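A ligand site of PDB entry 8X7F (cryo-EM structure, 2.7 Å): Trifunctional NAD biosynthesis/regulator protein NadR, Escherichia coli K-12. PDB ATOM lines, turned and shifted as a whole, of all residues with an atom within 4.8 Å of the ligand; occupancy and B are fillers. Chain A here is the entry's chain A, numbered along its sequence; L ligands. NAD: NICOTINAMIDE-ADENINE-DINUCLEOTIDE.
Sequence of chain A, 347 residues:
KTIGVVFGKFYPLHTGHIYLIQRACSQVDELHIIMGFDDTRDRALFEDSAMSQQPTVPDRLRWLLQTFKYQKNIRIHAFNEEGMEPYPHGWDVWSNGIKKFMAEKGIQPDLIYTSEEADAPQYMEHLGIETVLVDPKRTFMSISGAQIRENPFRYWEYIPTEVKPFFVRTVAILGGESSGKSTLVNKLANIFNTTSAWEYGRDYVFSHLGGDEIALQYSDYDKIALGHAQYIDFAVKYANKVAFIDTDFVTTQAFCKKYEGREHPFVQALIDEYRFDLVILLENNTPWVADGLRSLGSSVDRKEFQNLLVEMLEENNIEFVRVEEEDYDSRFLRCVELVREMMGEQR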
ATOM      1  N   PHE A   7      13.419  21.273 -24.755  1.00  0.00           N
ATOM      2  CA  PHE A   7      14.064  22.314 -23.979  1.00  0.00           C
ATOM      3  C   PHE A   7      14.877  21.677 -22.856  1.00  0.00           C
ATOM      4  O   PHE A   7      14.491  20.657 -22.282  1.00  0.00           O
ATOM      5  CB  PHE A   7      13.044  23.276 -23.365  1.00  0.00           C
ATOM      6  CG  PHE A   7      12.263  24.048 -24.382  1.00  0.00           C
ATOM      7  CD1 PHE A   7      12.862  25.031 -25.147  1.00  0.00           C
ATOM      8  CD2 PHE A   7      10.917  23.790 -24.567  1.00  0.00           C
ATOM      9  CE1 PHE A   7      12.136  25.746 -26.077  1.00  0.00           C
ATOM     10  CE2 PHE A   7      10.180  24.499 -25.503  1.00  0.00           C
ATOM     11  CZ  PHE A   7      10.797  25.477 -26.260  1.00  0.00           C
ATOM     12  N   GLY A   8      16.024  22.285 -22.560  1.00  0.00           N
ATOM     13  CA  GLY A   8      16.836  21.747 -21.491  1.00  0.00           C
ATOM     14  C   GLY A   8      18.080  22.557 -21.159  1.00  0.00           C
ATOM     15  O   GLY A   8      18.705  23.143 -22.041  1.00  0.00           O
ATOM     16  N   LYS A   9      18.429  22.578 -19.877  1.00  0.00           N
ATOM     17  CA  LYS A   9      19.690  23.181 -19.455  1.00  0.00           C
ATOM     18  C   LYS A   9      20.864  22.317 -19.884  1.00  0.00           C
ATOM     19  O   LYS A   9      21.933  22.855 -20.217  1.00  0.00           O
ATOM     20  CB  LYS A   9      19.667  23.400 -17.947  1.00  0.00           C
ATOM     21  CG  LYS A   9      20.906  24.075 -17.377  1.00  0.00           C
ATOM     22  CD  LYS A   9      21.027  23.813 -15.882  1.00  0.00           C
ATOM     23  CE  LYS A   9      20.931  22.327 -15.573  1.00  0.00           C
ATOM     24  NZ  LYS A   9      21.131  22.061 -14.127  1.00  0.00           N
ATOM     25  N   PHE A  10      20.699  21.000 -19.878  1.00  0.00           N
ATOM     26  CA  PHE A  10      21.702  20.042 -20.376  1.00  0.00           C
ATOM     27  C   PHE A  10      23.068  20.298 -19.761  1.00  0.00           C
ATOM     28  O   PHE A  10      24.096  20.271 -20.441  1.00  0.00           O
ATOM     29  CB  PHE A  10      21.800  20.088 -21.906  1.00  0.00           C
ATOM     30  CG  PHE A  10      20.513  19.743 -22.608  1.00  0.00           C
ATOM     31  CD1 PHE A  10      19.850  18.559 -22.349  1.00  0.00           C
ATOM     32  CD2 PHE A  10      19.977  20.609 -23.541  1.00  0.00           C
ATOM     33  CE1 PHE A  10      18.672  18.249 -22.989  1.00  0.00           C
ATOM     34  CE2 PHE A  10      18.796  20.303 -24.194  1.00  0.00           C
ATOM     35  CZ  PHE A  10      18.147  19.122 -23.916  1.00  0.00           C
ATOM     36  N   TYR A  11      23.090  20.550 -18.452  1.00  0.00           N
ATOM     37  CA  TYR A  11      24.309  20.997 -17.804  1.00  0.00           C
ATOM     38  C   TYR A  11      24.615  20.119 -16.604  1.00  0.00           C
ATOM     39  O   TYR A  11      24.207  20.448 -15.480  1.00  0.00           O
ATOM     40  CB  TYR A  11      24.174  22.464 -17.372  1.00  0.00           C
ATOM     41  CG  TYR A  11      25.404  23.037 -16.733  1.00  0.00           C
ATOM     42  CD1 TYR A  11      26.497  23.389 -17.502  1.00  0.00           C
ATOM     43  CD2 TYR A  11      25.487  23.216 -15.358  1.00  0.00           C
ATOM     44  CE1 TYR A  11      27.629  23.917 -16.931  1.00  0.00           C
ATOM     45  CE2 TYR A  11      26.624  23.740 -14.774  1.00  0.00           C
ATOM     46  CZ  TYR A  11      27.695  24.085 -15.578  1.00  0.00           C
ATOM     47  OH  TYR A  11      28.834  24.606 -15.027  1.00  0.00           O
ATOM     48  N   HIS A  14      23.524  14.012 -20.029  1.00  0.00           N
ATOM     49  CA  HIS A  14      23.712  12.628 -19.615  1.00  0.00           C
ATOM     50  C   HIS A  14      22.797  11.727 -20.428  1.00  0.00           C
ATOM     51  O   HIS A  14      22.032  12.188 -21.281  1.00  0.00           O
ATOM     52  CB  HIS A  14      23.478  12.459 -18.105  1.00  0.00           C
ATOM     53  CG  HIS A  14      22.140  12.933 -17.628  1.00  0.00           C
ATOM     54  ND1 HIS A  14      20.961  12.316 -17.987  1.00  0.00           N
ATOM     55  CD2 HIS A  14      21.798  13.962 -16.815  1.00  0.00           C
ATOM     56  CE1 HIS A  14      19.953  12.939 -17.420  1.00  0.00           C
ATOM     57  NE2 HIS A  14      20.428  13.938 -16.704  1.00  0.00           N
ATOM     58  N   GLY A  16      20.173  10.031 -19.778  1.00  0.00           N
ATOM     59  CA  GLY A  16      18.739  10.243 -19.708  1.00  0.00           C
ATOM     60  C   GLY A  16      18.256  11.230 -20.743  1.00  0.00           C
ATOM     61  O   GLY A  16      17.233  11.009 -21.404  1.00  0.00           O
ATOM     62  N   HIS A  17      18.991  12.326 -20.922  1.00  0.00           N
ATOM     63  CA  HIS A  17      18.682  13.274 -21.988  1.00  0.00           C
ATOM     64  C   HIS A  17      18.820  12.624 -23.357  1.00  0.00           C
ATOM     65  O   HIS A  17      18.008  12.885 -24.254  1.00  0.00           O
ATOM     66  CB  HIS A  17      19.607  14.489 -21.893  1.00  0.00           C
ATOM     67  CG  HIS A  17      19.480  15.255 -20.614  1.00  0.00           C
ATOM     68  ND1 HIS A  17      20.576  15.691 -19.905  1.00  0.00           N
ATOM     69  CD2 HIS A  17      18.402  15.670 -19.921  1.00  0.00           C
ATOM     70  CE1 HIS A  17      20.171  16.338 -18.832  1.00  0.00           C
ATOM     71  NE2 HIS A  17      18.852  16.338 -18.816  1.00  0.00           N
ATOM     72  N   LEU A  20      15.820  10.441 -23.917  1.00  0.00           N
ATOM     73  CA  LEU A  20      14.696  11.314 -24.243  1.00  0.00           C
ATOM     74  C   LEU A  20      14.744  11.770 -25.690  1.00  0.00           C
ATOM     75  O   LEU A  20      13.769  11.645 -26.436  1.00  0.00           O
ATOM     76  CB  LEU A  20      14.699  12.535 -23.315  1.00  0.00           C
ATOM     77  CG  LEU A  20      13.569  13.551 -23.497  1.00  0.00           C
ATOM     78  CD1 LEU A  20      12.224  12.942 -23.191  1.00  0.00           C
ATOM     79  CD2 LEU A  20      13.808  14.786 -22.649  1.00  0.00           C
ATOM     80  N   GLY A  36      18.944  27.152 -23.382  1.00  0.00           N
ATOM     81  CA  GLY A  36      19.050  28.470 -22.782  1.00  0.00           C
ATOM     82  C   GLY A  36      20.204  28.559 -21.803  1.00  0.00           C
ATOM     83  O   GLY A  36      20.518  27.609 -21.098  1.00  0.00           O
ATOM     84  N   ARG A  41      24.187  32.513 -13.500  1.00  0.00           N
ATOM     85  CA  ARG A  41      23.646  31.274 -12.972  1.00  0.00           C
ATOM     86  C   ARG A  41      24.520  30.086 -13.333  1.00  0.00           C
ATOM     87  O   ARG A  41      24.811  29.222 -12.490  1.00  0.00           O
ATOM     88  CB  ARG A  41      22.213  31.077 -13.475  1.00  0.00           C
ATOM     89  CG  ARG A  41      21.539  29.798 -13.010  1.00  0.00           C
ATOM     90  CD  ARG A  41      20.521  29.311 -14.027  1.00  0.00           C
ATOM     91  NE  ARG A  41      21.137  28.558 -15.110  1.00  0.00           N
ATOM     92  CZ  ARG A  41      20.576  28.345 -16.293  1.00  0.00           C
ATOM     93  NH1 ARG A  41      19.383  28.845 -16.588  1.00  0.00           N
ATOM     94  NH2 ARG A  41      21.229  27.634 -17.203  1.00  0.00           N
ATOM     95  N   GLU A  81      18.810  34.207 -21.808  1.00  0.00           N
ATOM     96  CA  GLU A  81      17.708  34.506 -20.897  1.00  0.00           C
ATOM     97  C   GLU A  81      18.161  35.436 -19.783  1.00  0.00           C
ATOM     98  O   GLU A  81      17.755  35.292 -18.630  1.00  0.00           O
ATOM     99  CB  GLU A  81      17.125  33.228 -20.306  1.00  0.00           C
ATOM    100  CG  GLU A  81      18.174  32.260 -19.760  1.00  0.00           C
ATOM    101  CD  GLU A  81      17.560  31.148 -18.932  1.00  0.00           C
ATOM    102  OE1 GLU A  81      16.820  31.445 -17.983  1.00  0.00           O
ATOM    103  OE2 GLU A  81      17.835  29.966 -19.236  1.00  0.00           O
ATOM    104  N   GLU A  85      13.385  36.418 -14.193  1.00  0.00           N
ATOM    105  CA  GLU A  85      13.192  35.826 -12.876  1.00  0.00           C
ATOM    106  C   GLU A  85      13.429  34.323 -12.931  1.00  0.00           C
ATOM    107  O   GLU A  85      13.051  33.669 -13.908  1.00  0.00           O
ATOM    108  CB  GLU A  85      11.785  36.115 -12.361  1.00  0.00           C
ATOM    109  CG  GLU A  85      11.509  37.585 -12.069  1.00  0.00           C
ATOM    110  CD  GLU A  85      12.192  38.067 -10.805  1.00  0.00           C
ATOM    111  OE1 GLU A  85      12.470  37.226  -9.920  1.00  0.00           O
ATOM    112  OE2 GLU A  85      12.441  39.283 -10.693  1.00  0.00           O
ATOM    113  N   PRO A  86      14.091  33.751 -11.933  1.00  0.00           N
ATOM    114  CA  PRO A  86      14.344  32.312 -11.925  1.00  0.00           C
ATOM    115  C   PRO A  86      13.076  31.483 -12.046  1.00  0.00           C
ATOM    116  O   PRO A  86      11.959  31.942 -11.809  1.00  0.00           O
ATOM    117  CB  PRO A  86      15.004  32.099 -10.566  1.00  0.00           C
ATOM    118  CG  PRO A  86      15.794  33.370 -10.338  1.00  0.00           C
ATOM    119  CD  PRO A  86      15.219  34.449 -11.281  1.00  0.00           C
ATOM    120  N   TYR A  87      13.269  30.223 -12.427  1.00  0.00           N
ATOM    121  CA  TYR A  87      12.204  29.244 -12.421  1.00  0.00           C
ATOM    122  C   TYR A  87      11.739  29.005 -10.984  1.00  0.00           C
ATOM    123  O   TYR A  87      12.555  28.968 -10.061  1.00  0.00           O
ATOM    124  CB  TYR A  87      12.696  27.931 -13.042  1.00  0.00           C
ATOM    125  CG  TYR A  87      11.691  26.795 -13.053  1.00  0.00           C
ATOM    126  CD1 TYR A  87      10.744  26.703 -14.063  1.00  0.00           C
ATOM    127  CD2 TYR A  87      11.709  25.825 -12.072  1.00  0.00           C
ATOM    128  CE1 TYR A  87       9.822  25.668 -14.083  1.00  0.00           C
ATOM    129  CE2 TYR A  87      10.792  24.786 -12.079  1.00  0.00           C
ATOM    130  CZ  TYR A  87       9.858  24.709 -13.080  1.00  0.00           C
ATOM    131  OH  TYR A  87       8.947  23.681 -13.094  1.00  0.00           O
ATOM    132  N   HIS A  89       9.214  31.296 -11.160  1.00  0.00           N
ATOM    133  CA  HIS A  89       8.560  32.608 -11.166  1.00  0.00           C
ATOM    134  C   HIS A  89       8.665  33.265 -12.541  1.00  0.00           C
ATOM    135  O   HIS A  89       7.776  34.022 -12.936  1.00  0.00           O
ATOM    136  CB  HIS A  89       9.163  33.493 -10.085  1.00  0.00           C
ATOM    137  CG  HIS A  89       9.362  32.789  -8.777  1.00  0.00           C
ATOM    138  ND1 HIS A  89      10.608  32.516  -8.260  1.00  0.00           N
ATOM    139  CD2 HIS A  89       8.476  32.289  -7.890  1.00  0.00           C
ATOM    140  CE1 HIS A  89      10.486  31.878  -7.106  1.00  0.00           C
ATOM    141  NE2 HIS A  89       9.196  31.728  -6.861  1.00  0.00           N
ATOM    142  N   GLY A  90       9.737  32.988 -13.272  1.00  0.00           N
ATOM    143  CA  GLY A  90       9.914  33.563 -14.589  1.00  0.00           C
ATOM    144  C   GLY A  90       9.306  32.751 -15.707  1.00  0.00           C
ATOM    145  O   GLY A  90       9.967  32.476 -16.716  1.00  0.00           O
ATOM    146  N   TRP A  91       8.045  32.354 -15.552  1.00  0.00           N
ATOM    147  CA  TRP A  91       7.326  31.606 -16.581  1.00  0.00           C
ATOM    148  C   TRP A  91       6.673  32.499 -17.639  1.00  0.00           C
ATOM    149  O   TRP A  91       6.043  31.966 -18.555  1.00  0.00           O
ATOM    150  CB  TRP A  91       6.266  30.713 -15.948  1.00  0.00           C
ATOM    151  CG  TRP A  91       6.693  29.301 -15.699  1.00  0.00           C
ATOM    152  CD1 TRP A  91       6.955  28.725 -14.486  1.00  0.00           C
ATOM    153  CD2 TRP A  91       6.883  28.274 -16.680  1.00  0.00           C
ATOM    154  NE1 TRP A  91       7.308  27.408 -14.658  1.00  0.00           N
ATOM    155  CE2 TRP A  91       7.270  27.103 -15.995  1.00  0.00           C
ATOM    156  CE3 TRP A  91       6.772  28.232 -18.070  1.00  0.00           C
ATOM    157  CZ2 TRP A  91       7.543  25.910 -16.653  1.00  0.00           C
ATOM    158  CZ3 TRP A  91       7.043  27.046 -18.717  1.00  0.00           C
ATOM    159  CH2 TRP A  91       7.432  25.903 -18.015  1.00  0.00           C
ATOM    160  N   TRP A  94      10.318  34.458 -19.868  1.00  0.00           N
ATOM    161  CA  TRP A  94      11.019  33.401 -20.581  1.00  0.00           C
ATOM    162  C   TRP A  94      10.210  32.915 -21.774  1.00  0.00           C
ATOM    163  O   TRP A  94      10.766  32.658 -22.845  1.00  0.00           O
ATOM    164  CB  TRP A  94      11.333  32.247 -19.625  1.00  0.00           C
ATOM    165  CG  TRP A  94      12.012  31.072 -20.276  1.00  0.00           C
ATOM    166  CD1 TRP A  94      13.360  30.842 -20.325  1.00  0.00           C
ATOM    167  CD2 TRP A  94      11.392  29.982 -20.968  1.00  0.00           C
ATOM    168  NE1 TRP A  94      13.610  29.667 -20.992  1.00  0.00           N
ATOM    169  CE2 TRP A  94      12.420  29.119 -21.403  1.00  0.00           C
ATOM    170  CE3 TRP A  94      10.063  29.650 -21.246  1.00  0.00           C
ATOM    171  CZ2 TRP A  94      12.159  27.955 -22.103  1.00  0.00           C
ATOM    172  CZ3 TRP A  94       9.807  28.488 -21.955  1.00  0.00           C
ATOM    173  CH2 TRP A  94      10.850  27.650 -22.379  1.00  0.00           C
ATOM    174  N   THR A 114       9.050  16.341 -23.404  1.00  0.00           N
ATOM    175  CA  THR A 114       9.538  16.614 -22.068  1.00  0.00           C
ATOM    176  C   THR A 114       9.326  15.384 -21.199  1.00  0.00           C
ATOM    177  O   THR A 114       8.568  14.472 -21.536  1.00  0.00           O
ATOM    178  CB  THR A 114       8.843  17.833 -21.451  1.00  0.00           C
ATOM    179  OG1 THR A 114       9.439  18.155 -20.189  1.00  0.00           O
ATOM    180  CG2 THR A 114       7.357  17.555 -21.246  1.00  0.00           C
ATOM    181  N   SER A 115      10.021  15.357 -20.054  1.00  0.00           N
ATOM    182  CA  SER A 115       9.895  14.265 -19.097  1.00  0.00           C
ATOM    183  C   SER A 115       9.554  14.783 -17.705  1.00  0.00           C
ATOM    184  O   SER A 115       9.949  14.181 -16.701  1.00  0.00           O
ATOM    185  CB  SER A 115      11.172  13.434 -19.049  1.00  0.00           C
ATOM    186  OG  SER A 115      11.234  12.665 -17.866  1.00  0.00           O
ATOM    187  N   GLU A 116       8.817  15.890 -17.627  1.00  0.00           N
ATOM    188  CA  GLU A 116       8.316  16.411 -16.362  1.00  0.00           C
ATOM    189  C   GLU A 116       6.800  16.465 -16.427  1.00  0.00           C
ATOM    190  O   GLU A 116       6.227  17.115 -17.311  1.00  0.00           O
ATOM    191  CB  GLU A 116       8.879  17.810 -16.072  1.00  0.00           C
ATOM    192  CG  GLU A 116      10.379  17.925 -16.273  1.00  0.00           C
ATOM    193  CD  GLU A 116      11.175  17.139 -15.250  1.00  0.00           C
ATOM    194  OE1 GLU A 116      10.678  16.975 -14.112  1.00  0.00           O
ATOM    195  OE2 GLU A 116      12.290  16.683 -15.578  1.00  0.00           O
ATOM    196  N   TYR A 123       3.784  24.524 -19.984  1.00  0.00           N
ATOM    197  CA  TYR A 123       4.152  24.526 -21.406  1.00  0.00           C
ATOM    198  C   TYR A 123       2.926  24.719 -22.276  1.00  0.00           C
ATOM    199  O   TYR A 123       2.914  25.555 -23.195  1.00  0.00           O
ATOM    200  CB  TYR A 123       4.856  23.219 -21.782  1.00  0.00           C
ATOM    201  CG  TYR A 123       6.318  23.136 -21.398  1.00  0.00           C
ATOM    202  CD1 TYR A 123       7.225  24.109 -21.814  1.00  0.00           C
ATOM    203  CD2 TYR A 123       6.797  22.069 -20.661  1.00  0.00           C
ATOM    204  CE1 TYR A 123       8.558  24.022 -21.474  1.00  0.00           C
ATOM    205  CE2 TYR A 123       8.130  21.982 -20.321  1.00  0.00           C
ATOM    206  CZ  TYR A 123       9.010  22.959 -20.727  1.00  0.00           C
ATOM    207  OH  TYR A 123      10.337  22.861 -20.381  1.00  0.00           O
ATOM    208  N   VAL A 134       7.646  11.502 -21.983  1.00  0.00           N
ATOM    209  CA  VAL A 134       8.448  10.334 -22.321  1.00  0.00           C
ATOM    210  C   VAL A 134       9.111   9.837 -21.049  1.00  0.00           C
ATOM    211  O   VAL A 134       9.815  10.598 -20.378  1.00  0.00           O
ATOM    212  CB  VAL A 134       9.501  10.660 -23.398  1.00  0.00           C
ATOM    213  CG1 VAL A 134      10.571   9.574 -23.462  1.00  0.00           C
ATOM    214  CG2 VAL A 134       8.837  10.831 -24.755  1.00  0.00           C
ATOM    215  N   ASP A 135       8.894   8.562 -20.724  1.00  0.00           N
ATOM    216  CA  ASP A 135       9.451   7.941 -19.537  1.00  0.00           C
ATOM    217  C   ASP A 135       9.176   8.762 -18.268  1.00  0.00           C
ATOM    218  O   ASP A 135      10.111   9.174 -17.578  1.00  0.00           O
ATOM    219  CB  ASP A 135      10.938   7.690 -19.699  1.00  0.00           C
ATOM    220  CG  ASP A 135      11.466   6.608 -18.781  1.00  0.00           C
ATOM    221  OD1 ASP A 135      10.656   5.772 -18.327  1.00  0.00           O
ATOM    222  OD2 ASP A 135      12.681   6.586 -18.513  1.00  0.00           O
ATOM    223  N   ARG A 138      10.880   7.607 -15.137  1.00  0.00           N
ATOM    224  CA  ARG A 138      12.335   7.496 -15.203  1.00  0.00           C
ATOM    225  C   ARG A 138      12.790   6.051 -15.014  1.00  0.00           C
ATOM    226  O   ARG A 138      13.676   5.746 -14.210  1.00  0.00           O
ATOM    227  CB  ARG A 138      13.003   8.426 -14.183  1.00  0.00           C
ATOM    228  CG  ARG A 138      12.487   9.855 -14.225  1.00  0.00           C
ATOM    229  CD  ARG A 138      12.759  10.502 -15.573  1.00  0.00           C
ATOM    230  NE  ARG A 138      12.414  11.916 -15.575  1.00  0.00           N
ATOM    231  CZ  ARG A 138      13.141  12.879 -15.008  1.00  0.00           C
ATOM    232  NH1 ARG A 138      14.255  12.598 -14.357  1.00  0.00           N
ATOM    233  NH2 ARG A 138      12.735  14.137 -15.088  1.00  0.00           N
ATOM    234  N   MET A 141      16.552   5.548 -16.806  1.00  0.00           N
ATOM    235  CA  MET A 141      17.580   6.194 -15.998  1.00  0.00           C
ATOM    236  C   MET A 141      16.915   6.966 -14.868  1.00  0.00           C
ATOM    237  O   MET A 141      15.947   7.684 -15.094  1.00  0.00           O
ATOM    238  CB  MET A 141      18.448   7.136 -16.825  1.00  0.00           C
ATOM    239  CG  MET A 141      19.577   7.769 -16.046  1.00  0.00           C
ATOM    240  SD  MET A 141      20.649   8.809 -17.048  1.00  0.00           S
ATOM    241  CE  MET A 141      21.760   9.448 -15.801  1.00  0.00           C
ATOM    242  N   ILE A 143      19.102   8.583 -12.352  1.00  0.00           N
ATOM    243  CA  ILE A 143      20.068   9.535 -11.811  1.00  0.00           C
ATOM    244  C   ILE A 143      19.764  10.931 -12.339  1.00  0.00           C
ATOM    245  O   ILE A 143      19.391  11.106 -13.501  1.00  0.00           O
ATOM    246  CB  ILE A 143      21.501   9.109 -12.187  1.00  0.00           C
ATOM    247  CG1 ILE A 143      21.638   7.589 -12.058  1.00  0.00           C
ATOM    248  CG2 ILE A 143      22.512   9.811 -11.299  1.00  0.00           C
ATOM    249  CD1 ILE A 143      21.596   7.076 -10.640  1.00  0.00           C
HETATM  250  PA  NAD L   1      17.348  19.667 -17.662  1.00  0.00           P
HETATM  251  O1A NAD L   1      18.677  19.331 -18.293  1.00  0.00           O
HETATM  252  O2A NAD L   1      17.339  19.156 -16.237  1.00  0.00           O
HETATM  253  O5B NAD L   1      16.126  18.967 -18.510  1.00  0.00           O
HETATM  254  C5B NAD L   1      16.322  18.604 -19.850  1.00  0.00           C
HETATM  255  C4B NAD L   1      15.134  17.688 -20.306  1.00  0.00           C
HETATM  256  O4B NAD L   1      15.474  16.460 -20.209  1.00  0.00           O
HETATM  257  C3B NAD L   1      13.913  17.863 -19.350  1.00  0.00           C
HETATM  258  O3B NAD L   1      12.770  17.852 -20.073  1.00  0.00           O
HETATM  259  C2B NAD L   1      13.967  16.652 -18.444  1.00  0.00           C
HETATM  260  O2B NAD L   1      12.579  16.296 -17.985  1.00  0.00           O
HETATM  261  C1B NAD L   1      14.444  15.718 -19.207  1.00  0.00           C
HETATM  262  N9A NAD L   1      15.130  14.721 -18.421  1.00  0.00           N
HETATM  263  C8A NAD L   1      16.015  14.950 -17.479  1.00  0.00           C
HETATM  264  N7A NAD L   1      16.438  13.809 -16.975  1.00  0.00           N
HETATM  265  C5A NAD L   1      15.814  12.803 -17.621  1.00  0.00           C
HETATM  266  C6A NAD L   1      15.864  11.403 -17.518  1.00  0.00           C
HETATM  267  N6A NAD L   1      16.732  10.753 -16.551  1.00  0.00           N
HETATM  268  N1A NAD L   1      15.092  10.670 -18.322  1.00  0.00           N
HETATM  269  C2A NAD L   1      14.299  11.268 -19.191  1.00  0.00           C
HETATM  270  N3A NAD L   1      14.231  12.582 -19.316  1.00  0.00           N
HETATM  271  C4A NAD L   1      14.976  13.393 -18.548  1.00  0.00           C
HETATM  272  O3  NAD L   1      17.130  21.295 -17.657  1.00  0.00           O
HETATM  273  PN  NAD L   1      15.701  22.050 -17.329  1.00  0.00           P
HETATM  274  O1N NAD L   1      15.631  22.408 -15.869  1.00  0.00           O
HETATM  275  O2N NAD L   1      14.543  21.154 -17.687  1.00  0.00           O
HETATM  276  O5D NAD L   1      15.623  23.434 -18.232  1.00  0.00           O
HETATM  277  C5D NAD L   1      14.431  23.724 -18.933  1.00  0.00           C
HETATM  278  C4D NAD L   1      14.500  25.026 -19.364  1.00  0.00           C
HETATM  279  O4D NAD L   1      13.148  25.723 -19.120  1.00  0.00           O
HETATM  280  C3D NAD L   1      15.529  25.843 -18.483  1.00  0.00           C
HETATM  281  O3D NAD L   1      16.847  25.920 -19.192  1.00  0.00           O
HETATM  282  C2D NAD L   1      15.037  27.000 -18.351  1.00  0.00           C
HETATM  283  O2D NAD L   1      15.775  27.943 -19.199  1.00  0.00           O
HETATM  284  C1D NAD L   1      13.433  26.948 -18.829  1.00  0.00           C
HETATM  285  N1N NAD L   1      12.573  27.402 -17.781  1.00  0.00           N
HETATM  286  C2N NAD L   1      13.176  28.620 -17.158  1.00  0.00           C
HETATM  287  C3N NAD L   1      12.203  29.787 -16.999  1.00  0.00           C
HETATM  288  C7N NAD L   1      12.802  30.808 -15.988  1.00  0.00           C
HETATM  289  O7N NAD L   1      12.123  31.264 -15.131  1.00  0.00           O
HETATM  290  N7N NAD L   1      14.205  31.168 -16.076  1.00  0.00           N
HETATM  291  C4N NAD L   1      10.877  29.324 -16.502  1.00  0.00           C
HETATM  292  C5N NAD L   1      10.229  28.367 -17.436  1.00  0.00           C
HETATM  293  C6N NAD L   1      11.215  27.609 -18.353  1.00  0.00           C
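The backbone NH (N) of Glu 116 is in hydrogen-bond range of the side-chain hydroxyl (OG1) of Thr 114.
The side-chain carboxylate (OE2) of Glu 116 lies within salt-bridge range of the guanidinium group (NH2) of Arg 138 (2.6 Å).
The backbone carbonyl oxygen (O) of Glu 85 lies close to the backbone NH (N) of Gly 90 (3.4 Å).
The side-chain carboxylate (OE2) of Glu 81 lies within salt-bridge range of the guanidinium group (NH1) of Arg 41, 3.3 Å away.
N of His 14 lies within hydrogen-bond range of ND1 of His 17 (3.4 Å).
O of Thr 114 is in hydrogen-bond range of N of Val 134, 3.1 Å away.
The side-chain sulfur (SD) of Met 141 lies within hydrogen-bond range of a ring nitrogen (ND1) of His 14, at 3.6 Å.
The side-chain sulfur (SD) of Met 141 lies within hydrogen-bond range of the backbone NH (N) of Gly 16, at 3.0 Å.
The side-chain carboxylate (OE2) of Glu 116 is in hydrogen-bond range of an oxygen (O2B) of the ligand (2.5 Å).
The backbone NH (N) of Lys 9 sits at hydrogen-bond distance from an oxygen (O3) of the ligand, at 2.9 Å.
An oxygen (O2D) of the ligand lies within hydrogen-bond range of the side-chain carboxylate of Glu 81, 2.9 Å away.
The backbone NH of Gly 90 lies close to an oxygen (O7N) of the ligand (3.5 Å).
An oxygen (O1A) of the ligand is in hydrogen-bond range of a ring nitrogen (NE2) of His 17, at 3.0 Å.
An oxygen (O1A) of the ligand lies within hydrogen-bond range of the backbone NH (N) of Phe 10.
An oxygen (O7N) of the ligand lies within hydrogen-bond range of the backbone NH of Tyr 87 (3.1 Å).
The backbone NH (N) of Ser 115 lies close to an oxygen (O2B) of the ligand (3.4 Å).
OG of Ser 115 sits close to N3A of the ligand, at 3.3 Å.
NE1 of Trp 94 is in hydrogen-bond range of O2D of the ligand.
O3B of the ligand sits at hydrogen-bond distance from OG1 of Thr 114 (3.3 Å).
A nitrogen (N6A) of the ligand sits at hydrogen-bond distance from the backbone carbonyl oxygen (O) of Met 141 (3.5 Å).
O of Glu 85 lies close to O7N of the ligand, 2.9 Å away.
O7N of the ligand sits close to O of Pro 86 (3.4 Å).
Phe 7 touches the ligand (O to C4B, 3.6 Å).
CA of Gly 8 touches C5B of the ligand, 3.6 Å away.
His 14 touches the ligand.
Gly 16 touches the ligand.
Leu 20 touches the ligand (CD2 to O4B, 3.4 Å).
CD2 of Trp 91 touches C5N of the ligand, 3.4 Å away.
CD of Arg 138 touches N1A of the ligand (3.6 Å).
Hydrophobic or aromatic side chains that line the ligand: Phe 10, His 14, His 17, Leu 20, Tyr 87, Trp 91 and Trp 94.
The nearest printed residue that does not touch the ligand is Ile 143 (4.1 Å).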
